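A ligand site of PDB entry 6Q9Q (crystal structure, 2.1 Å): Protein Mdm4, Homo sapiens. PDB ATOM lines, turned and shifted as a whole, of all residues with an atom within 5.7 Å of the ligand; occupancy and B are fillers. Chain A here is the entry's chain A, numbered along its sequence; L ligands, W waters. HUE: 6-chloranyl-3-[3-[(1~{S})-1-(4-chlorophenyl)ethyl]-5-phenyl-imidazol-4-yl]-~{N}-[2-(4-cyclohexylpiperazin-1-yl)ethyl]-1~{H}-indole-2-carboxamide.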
ATOM      1  N   MET A  42      -7.405  23.844  17.057  1.00  0.00           N
ATOM      2  CA  MET A  42      -8.563  23.881  16.152  1.00  0.00           C
ATOM      3  C   MET A  42      -8.874  25.293  15.664  1.00  0.00           C
ATOM      4  O   MET A  42      -9.223  25.485  14.492  1.00  0.00           O
ATOM      5  CB  MET A  42      -9.810  23.269  16.803  1.00  0.00           C
ATOM      6  CG  MET A  42      -9.661  21.809  17.226  1.00  0.00           C
ATOM      7  SD  MET A  42      -8.807  20.785  16.015  1.00  0.00           S
ATOM      8  CE  MET A  42      -9.958  20.767  14.634  1.00  0.00           C
ATOM      9  N   HIS A  43      -8.766  26.277  16.561  1.00  0.00           N
ATOM     10  CA  HIS A  43      -8.937  27.672  16.166  1.00  0.00           C
ATOM     11  C   HIS A  43      -7.917  28.049  15.095  1.00  0.00           C
ATOM     12  O   HIS A  43      -8.286  28.580  14.048  1.00  0.00           O
ATOM     13  CB  HIS A  43      -8.802  28.614  17.360  1.00  0.00           C
ATOM     14  CG  HIS A  43      -8.629  30.058  16.973  1.00  0.00           C
ATOM     15  ND1 HIS A  43      -9.677  30.847  16.565  1.00  0.00           N
ATOM     16  CD2 HIS A  43      -7.526  30.836  16.917  1.00  0.00           C
ATOM     17  CE1 HIS A  43      -9.230  32.057  16.280  1.00  0.00           C
ATOM     18  NE2 HIS A  43      -7.924  32.069  16.479  1.00  0.00           N
ATOM     19  N   LEU A  45      -6.061  26.164  13.126  1.00  0.00           N
ATOM     20  CA  LEU A  45      -6.227  25.388  11.889  1.00  0.00           C
ATOM     21  C   LEU A  45      -7.307  26.014  11.004  1.00  0.00           C
ATOM     22  O   LEU A  45      -7.133  26.125   9.802  1.00  0.00           O
ATOM     23  CB  LEU A  45      -6.544  23.906  12.192  1.00  0.00           C
ATOM     24  CG  LEU A  45      -5.339  23.037  12.600  1.00  0.00           C
ATOM     25  CD1 LEU A  45      -5.753  21.621  12.994  1.00  0.00           C
ATOM     26  CD2 LEU A  45      -4.317  22.987  11.486  1.00  0.00           C
ATOM     27  N   GLY A  46      -8.428  26.412  11.606  1.00  0.00           N
ATOM     28  CA  GLY A  46      -9.458  27.179  10.898  1.00  0.00           C
ATOM     29  C   GLY A  46      -8.907  28.452  10.283  1.00  0.00           C
ATOM     30  O   GLY A  46      -9.194  28.763   9.130  1.00  0.00           O
ATOM     31  N   GLN A  47      -8.080  29.165  11.043  1.00  0.00           N
ATOM     32  CA  GLN A  47      -7.448  30.386  10.571  1.00  0.00           C
ATOM     33  C   GLN A  47      -6.468  30.108   9.440  1.00  0.00           C
ATOM     34  O   GLN A  47      -6.393  30.873   8.502  1.00  0.00           O
ATOM     35  CB  GLN A  47      -6.771  31.133  11.712  1.00  0.00           C
ATOM     36  CG  GLN A  47      -7.749  31.802  12.673  1.00  0.00           C
ATOM     37  CD  GLN A  47      -8.352  33.089  12.121  1.00  0.00           C
ATOM     38  OE1 GLN A  47      -9.314  33.058  11.345  1.00  0.00           O
ATOM     39  NE2 GLN A  47      -7.785  34.220  12.517  1.00  0.00           N
ATOM     40  N   ILE A  49      -6.702  27.670   7.234  1.00  0.00           N
ATOM     41  CA  ILE A  49      -7.527  27.427   6.062  1.00  0.00           C
ATOM     42  C   ILE A  49      -7.970  28.741   5.384  1.00  0.00           C
ATOM     43  O   ILE A  49      -7.954  28.838   4.148  1.00  0.00           O
ATOM     44  CB  ILE A  49      -8.730  26.513   6.411  1.00  0.00           C
ATOM     45  CG1 ILE A  49      -8.205  25.111   6.802  1.00  0.00           C
ATOM     46  CG2 ILE A  49      -9.718  26.448   5.222  1.00  0.00           C
ATOM     47  CD1 ILE A  49      -9.132  24.294   7.709  1.00  0.00           C
ATOM     48  N   MET A  50      -8.320  29.741   6.199  1.00  0.00           N
ATOM     49  CA  MET A  50      -8.653  31.093   5.710  1.00  0.00           C
ATOM     50  C   MET A  50      -7.476  31.750   4.996  1.00  0.00           C
ATOM     51  O   MET A  50      -7.623  32.201   3.863  1.00  0.00           O
ATOM     52  CB  MET A  50      -9.062  32.035   6.848  1.00  0.00           C
ATOM     53  CG  MET A  50     -10.004  31.474   7.902  1.00  0.00           C
ATOM     54  SD  MET A  50     -11.719  31.944   7.672  1.00  0.00           S
ATOM     55  CE  MET A  50     -12.100  31.048   6.206  1.00  0.00           C
ATOM     56  N   TYR A  55     -10.533  26.783   1.306  1.00  0.00           N
ATOM     57  CA  TYR A  55     -11.956  26.510   1.230  1.00  0.00           C
ATOM     58  C   TYR A  55     -12.566  26.956  -0.105  1.00  0.00           C
ATOM     59  O   TYR A  55     -12.031  27.857  -0.772  1.00  0.00           O
ATOM     60  CB  TYR A  55     -12.688  27.150   2.398  1.00  0.00           C
ATOM     61  CG  TYR A  55     -12.698  28.667   2.392  1.00  0.00           C
ATOM     62  CD1 TYR A  55     -13.756  29.381   1.818  1.00  0.00           C
ATOM     63  CD2 TYR A  55     -11.659  29.393   2.972  1.00  0.00           C
ATOM     64  CE1 TYR A  55     -13.768  30.789   1.814  1.00  0.00           C
ATOM     65  CE2 TYR A  55     -11.667  30.799   2.980  1.00  0.00           C
ATOM     66  CZ  TYR A  55     -12.727  31.475   2.405  1.00  0.00           C
ATOM     67  OH  TYR A  55     -12.732  32.848   2.419  1.00  0.00           O
ATOM     68  N   GLN A  60     -18.632  26.579   1.002  1.00  0.00           N
ATOM     69  CA  GLN A  60     -17.730  27.021   2.063  1.00  0.00           C
ATOM     70  C   GLN A  60     -17.470  25.975   3.144  1.00  0.00           C
ATOM     71  O   GLN A  60     -16.616  26.169   4.013  1.00  0.00           O
ATOM     72  CB  GLN A  60     -18.208  28.347   2.673  1.00  0.00           C
ATOM     73  CG  GLN A  60     -18.442  29.425   1.623  1.00  0.00           C
ATOM     74  CD  GLN A  60     -18.453  30.832   2.207  1.00  0.00           C
ATOM     75  OE1 GLN A  60     -18.693  31.033   3.403  1.00  0.00           O
ATOM     76  NE2 GLN A  60     -18.177  31.826   1.355  1.00  0.00           N
ATOM     77  N   HIS A  61     -18.194  24.857   3.080  1.00  0.00           N
ATOM     78  CA  HIS A  61     -17.980  23.724   3.975  1.00  0.00           C
ATOM     79  C   HIS A  61     -16.864  22.807   3.462  1.00  0.00           C
ATOM     80  O   HIS A  61     -16.315  22.002   4.206  1.00  0.00           O
ATOM     81  CB  HIS A  61     -19.272  22.935   4.182  1.00  0.00           C
ATOM     82  CG  HIS A  61     -19.847  22.361   2.929  1.00  0.00           C
ATOM     83  ND1 HIS A  61     -19.681  21.046   2.564  1.00  0.00           N
ATOM     84  CD2 HIS A  61     -20.588  22.929   1.946  1.00  0.00           C
ATOM     85  CE1 HIS A  61     -20.293  20.820   1.414  1.00  0.00           C
ATOM     86  NE2 HIS A  61     -20.858  21.946   1.022  1.00  0.00           N
ATOM     87  N   VAL A  63     -13.142  21.942   1.993  1.00  0.00           N
ATOM     88  CA  VAL A  63     -11.742  22.368   2.027  1.00  0.00           C
ATOM     89  C   VAL A  63     -10.902  21.497   1.098  1.00  0.00           C
ATOM     90  O   VAL A  63     -10.962  20.256   1.168  1.00  0.00           O
ATOM     91  CB  VAL A  63     -11.167  22.317   3.462  1.00  0.00           C
ATOM     92  CG1 VAL A  63      -9.661  22.658   3.466  1.00  0.00           C
ATOM     93  CG2 VAL A  63     -11.943  23.261   4.397  1.00  0.00           C
ATOM     94  N   LEU A  70      -1.036  20.684   4.821  1.00  0.00           N
ATOM     95  CA  LEU A  70      -2.170  20.172   5.591  1.00  0.00           C
ATOM     96  C   LEU A  70      -2.753  18.883   4.979  1.00  0.00           C
ATOM     97  O   LEU A  70      -3.148  17.970   5.710  1.00  0.00           O
ATOM     98  CB  LEU A  70      -3.268  21.240   5.721  1.00  0.00           C
ATOM     99  CG  LEU A  70      -4.559  20.886   6.483  1.00  0.00           C
ATOM    100  CD1 LEU A  70      -4.280  20.544   7.949  1.00  0.00           C
ATOM    101  CD2 LEU A  70      -5.611  21.990   6.382  1.00  0.00           C
ATOM    102  N   PHE A  79     -11.799  17.624   2.287  1.00  0.00           N
ATOM    103  CA  PHE A  79     -12.691  17.217   3.358  1.00  0.00           C
ATOM    104  C   PHE A  79     -13.795  18.236   3.539  1.00  0.00           C
ATOM    105  O   PHE A  79     -13.664  19.388   3.109  1.00  0.00           O
ATOM    106  CB  PHE A  79     -11.948  16.973   4.679  1.00  0.00           C
ATOM    107  CG  PHE A  79     -11.314  18.218   5.284  1.00  0.00           C
ATOM    108  CD1 PHE A  79     -12.043  19.037   6.144  1.00  0.00           C
ATOM    109  CD2 PHE A  79      -9.987  18.530   5.018  1.00  0.00           C
ATOM    110  CE1 PHE A  79     -11.467  20.173   6.708  1.00  0.00           C
ATOM    111  CE2 PHE A  79      -9.402  19.672   5.572  1.00  0.00           C
ATOM    112  CZ  PHE A  79     -10.144  20.489   6.428  1.00  0.00           C
ATOM    113  N   VAL A  81     -16.051  20.242   6.413  1.00  0.00           N
ATOM    114  CA  VAL A  81     -16.003  20.650   7.829  1.00  0.00           C
ATOM    115  C   VAL A  81     -17.176  20.079   8.637  1.00  0.00           C
ATOM    116  O   VAL A  81     -17.181  20.157   9.863  1.00  0.00           O
ATOM    117  CB  VAL A  81     -15.904  22.182   7.999  1.00  0.00           C
ATOM    118  CG1 VAL A  81     -14.677  22.727   7.281  1.00  0.00           C
ATOM    119  CG2 VAL A  81     -17.159  22.869   7.495  1.00  0.00           C
ATOM    120  N   LYS A  82     -18.162  19.515   7.944  1.00  0.00           N
ATOM    121  CA  LYS A  82     -19.251  18.791   8.600  1.00  0.00           C
ATOM    122  C   LYS A  82     -18.769  17.408   9.035  1.00  0.00           C
ATOM    123  O   LYS A  82     -19.344  16.814   9.958  1.00  0.00           O
ATOM    124  CB  LYS A  82     -20.448  18.655   7.668  1.00  0.00           C
ATOM    125  CG  LYS A  82     -20.757  19.887   6.842  1.00  0.00           C
ATOM    126  CD  LYS A  82     -21.657  20.870   7.576  1.00  0.00           C
ATOM    127  CE  LYS A  82     -22.243  21.889   6.610  1.00  0.00           C
ATOM    128  NZ  LYS A  82     -22.924  21.231   5.442  1.00  0.00           N
ATOM    129  N   PRO A  84     -15.684  15.888  10.636  1.00  0.00           N
ATOM    130  CA  PRO A  84     -14.414  16.141  11.334  1.00  0.00           C
ATOM    131  C   PRO A  84     -13.569  14.884  11.606  1.00  0.00           C
ATOM    132  O   PRO A  84     -12.446  15.001  12.110  1.00  0.00           O
ATOM    133  CB  PRO A  84     -14.880  16.743  12.661  1.00  0.00           C
ATOM    134  CG  PRO A  84     -16.177  16.064  12.923  1.00  0.00           C
ATOM    135  CD  PRO A  84     -16.813  15.820  11.583  1.00  0.00           C
ATOM    136  N   LEU A  87      -9.920  14.650  10.604  1.00  0.00           N
ATOM    137  CA  LEU A  87      -9.180  15.711  11.282  1.00  0.00           C
ATOM    138  C   LEU A  87      -8.677  15.327  12.665  1.00  0.00           C
ATOM    139  O   LEU A  87      -7.520  15.559  13.002  1.00  0.00           O
ATOM    140  CB  LEU A  87     -10.010  16.993  11.353  1.00  0.00           C
ATOM    141  CG  LEU A  87      -9.772  18.041  10.274  1.00  0.00           C
ATOM    142  CD1 LEU A  87      -8.303  18.496  10.285  1.00  0.00           C
ATOM    143  CD2 LEU A  87     -10.192  17.551   8.890  1.00  0.00           C
ATOM    144  N   TYR A  88      -9.561  14.737  13.465  1.00  0.00           N
ATOM    145  CA  TYR A  88      -9.203  14.331  14.823  1.00  0.00           C
ATOM    146  C   TYR A  88      -8.238  13.156  14.865  1.00  0.00           C
ATOM    147  O   TYR A  88      -7.448  13.029  15.791  1.00  0.00           O
ATOM    148  CB  TYR A  88     -10.455  14.068  15.650  1.00  0.00           C
ATOM    149  CG  TYR A  88     -11.188  15.335  16.048  1.00  0.00           C
ATOM    150  CD1 TYR A  88     -10.767  16.093  17.151  1.00  0.00           C
ATOM    151  CD2 TYR A  88     -12.294  15.781  15.323  1.00  0.00           C
ATOM    152  CE1 TYR A  88     -11.427  17.259  17.509  1.00  0.00           C
ATOM    153  CE2 TYR A  88     -12.962  16.950  15.686  1.00  0.00           C
ATOM    154  CZ  TYR A  88     -12.529  17.689  16.779  1.00  0.00           C
ATOM    155  OH  TYR A  88     -13.194  18.841  17.136  1.00  0.00           O
HETATM  156  C2  HUE L   1     -10.414  22.617  10.790  1.00  0.00           C
HETATM  157  C3  HUE L   1     -10.299  23.610  11.772  1.00  0.00           C
HETATM  158  C41 HUE L   1     -14.849  21.263  12.085  1.00  0.00           C
HETATM  159  C43 HUE L   1     -13.782  21.067  12.963  1.00  0.00           C
HETATM  160  C44 HUE L   1     -13.414  22.050  13.875  1.00  0.00           C
HETATM  161  C46 HUE L   1     -14.124  23.256  13.914  1.00  0.00           C
HETATM  162  C49 HUE L   1     -13.124  27.205  13.400  1.00  0.00           C
HETATM  163  C53 HUE L   1     -14.730  29.084  13.712  1.00  0.00           C
HETATM  164  C56 HUE L   1     -16.106  29.406  13.072  1.00  0.00           C
HETATM  165  C60 HUE L   1     -17.208  29.385  10.811  1.00  0.00           C
HETATM  166  C11 HUE L   1     -12.637  23.360  10.141  1.00  0.00           C
HETATM  167  C13 HUE L   1     -11.554  22.487   9.979  1.00  0.00           C
HETATM  168  C15 HUE L   1     -14.746  25.682  11.058  1.00  0.00           C
HETATM  169  C17 HUE L   1     -16.884  25.640  11.006  1.00  0.00           C
HETATM  170  C20 HUE L   1     -15.092  26.143   9.836  1.00  0.00           C
HETATM  171  C21 HUE L   1     -14.327  26.649   8.636  1.00  0.00           C
HETATM  172  C22 HUE L   1     -13.062  27.245   8.749  1.00  0.00           C
HETATM  173  C24 HUE L   1     -12.398  27.702   7.594  1.00  0.00           C
HETATM  174  C26 HUE L   1     -13.011  27.567   6.346  1.00  0.00           C
HETATM  175  C28 HUE L   1     -14.276  26.972   6.233  1.00  0.00           C
HETATM  176  C30 HUE L   1     -14.932  26.520   7.378  1.00  0.00           C
HETATM  177 CL1  HUE L   1      -9.068  21.533  10.583  1.00  0.00          CL
HETATM  178  C5  HUE L   1     -11.388  24.466  11.909  1.00  0.00           C
HETATM  179  N6  HUE L   1     -11.535  25.477  12.756  1.00  0.00           N
HETATM  180  C8  HUE L   1     -12.693  26.063  12.594  1.00  0.00           C
HETATM  181  C9  HUE L   1     -13.389  25.465  11.602  1.00  0.00           C
HETATM  182  C10 HUE L   1     -12.518  24.345  11.112  1.00  0.00           C
HETATM  183  N16 HUE L   1     -15.851  25.392  11.749  1.00  0.00           N
HETATM  184  N19 HUE L   1     -16.524  26.094   9.895  1.00  0.00           N
HETATM  185  C32 HUE L   1     -15.913  24.812  13.106  1.00  0.00           C
HETATM  186  C34 HUE L   1     -17.351  24.802  13.707  1.00  0.00           C
HETATM  187  C38 HUE L   1     -15.194  23.467  13.041  1.00  0.00           C
HETATM  188  C39 HUE L   1     -15.551  22.466  12.119  1.00  0.00           C
HETATM  189 CL2  HUE L   1     -12.898  19.565  12.927  1.00  0.00          CL
HETATM  190  O50 HUE L   1     -12.470  27.440  14.406  1.00  0.00           O
HETATM  191  N51 HUE L   1     -14.190  27.938  12.998  1.00  0.00           N
HETATM  192  N59 HUE L   1     -15.970  29.646  11.609  1.00  0.00           N
HETATM  193  C63 HUE L   1     -16.986  29.589   9.284  1.00  0.00           C
HETATM  194  N66 HUE L   1     -16.262  30.857   8.979  1.00  0.00           N
HETATM  195  C67 HUE L   1     -15.051  31.024   9.814  1.00  0.00           C
HETATM  196  C70 HUE L   1     -15.425  30.987  11.310  1.00  0.00           C
HETATM  197  C73 HUE L   1     -15.942  31.283   7.572  1.00  0.00           C
HETATM  198  C75 HUE L   1     -15.950  30.084   6.580  1.00  0.00           C
HETATM  199  C78 HUE L   1     -15.302  30.500   5.217  1.00  0.00           C
HETATM  200  C81 HUE L   1     -15.952  31.781   4.619  1.00  0.00           C
HETATM  201  C84 HUE L   1     -16.139  32.931   5.652  1.00  0.00           C
HETATM  202  C87 HUE L   1     -16.815  32.434   6.963  1.00  0.00           C
HETATM  203  O   HOH W   1     -18.637  26.526   8.181  1.00  0.00           O
HETATM  204  O   HOH W   2     -10.791  29.487  13.336  1.00  0.00           O
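The backbone carbonyl oxygen (O) of Met 42 is in hydrogen-bond range of a nitrogen (N6) of the ligand (2.9 Å). A nitrogen (N6) of the ligand lies close to the backbone NH (N) of Gly 46, 3.4 Å away.
Residues that only touch the ligand: Gln 60 (3.1 Å), Leu 87 (3.1 Å), Met 50 (3.4 Å), Val 81 (3.4 Å), Pro 84 (3.5 Å), Ile 49 (3.7 Å), Tyr 55 (3.7 Å), Leu 45 (3.8 Å), Tyr 88 (3.8 Å) and His 43 (3.95 Å). Hydrophobic or aromatic side chains that line the ligand: Met 42, Leu 45, Ile 49, Met 50, Tyr 55, Val 81, Pro 84, Leu 87 and Tyr 88. Of the 18 residues printed, 12 come within 4 Å of the ligand.
Water W2 bridges O of His 43 (2.8 Å) and O50 of the ligand (2.9 Å).
The backbone NH (N) of Val 81 sits at hydrogen-bond distance from the backbone carbonyl oxygen (O) of His 61, 2.8 Å away.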
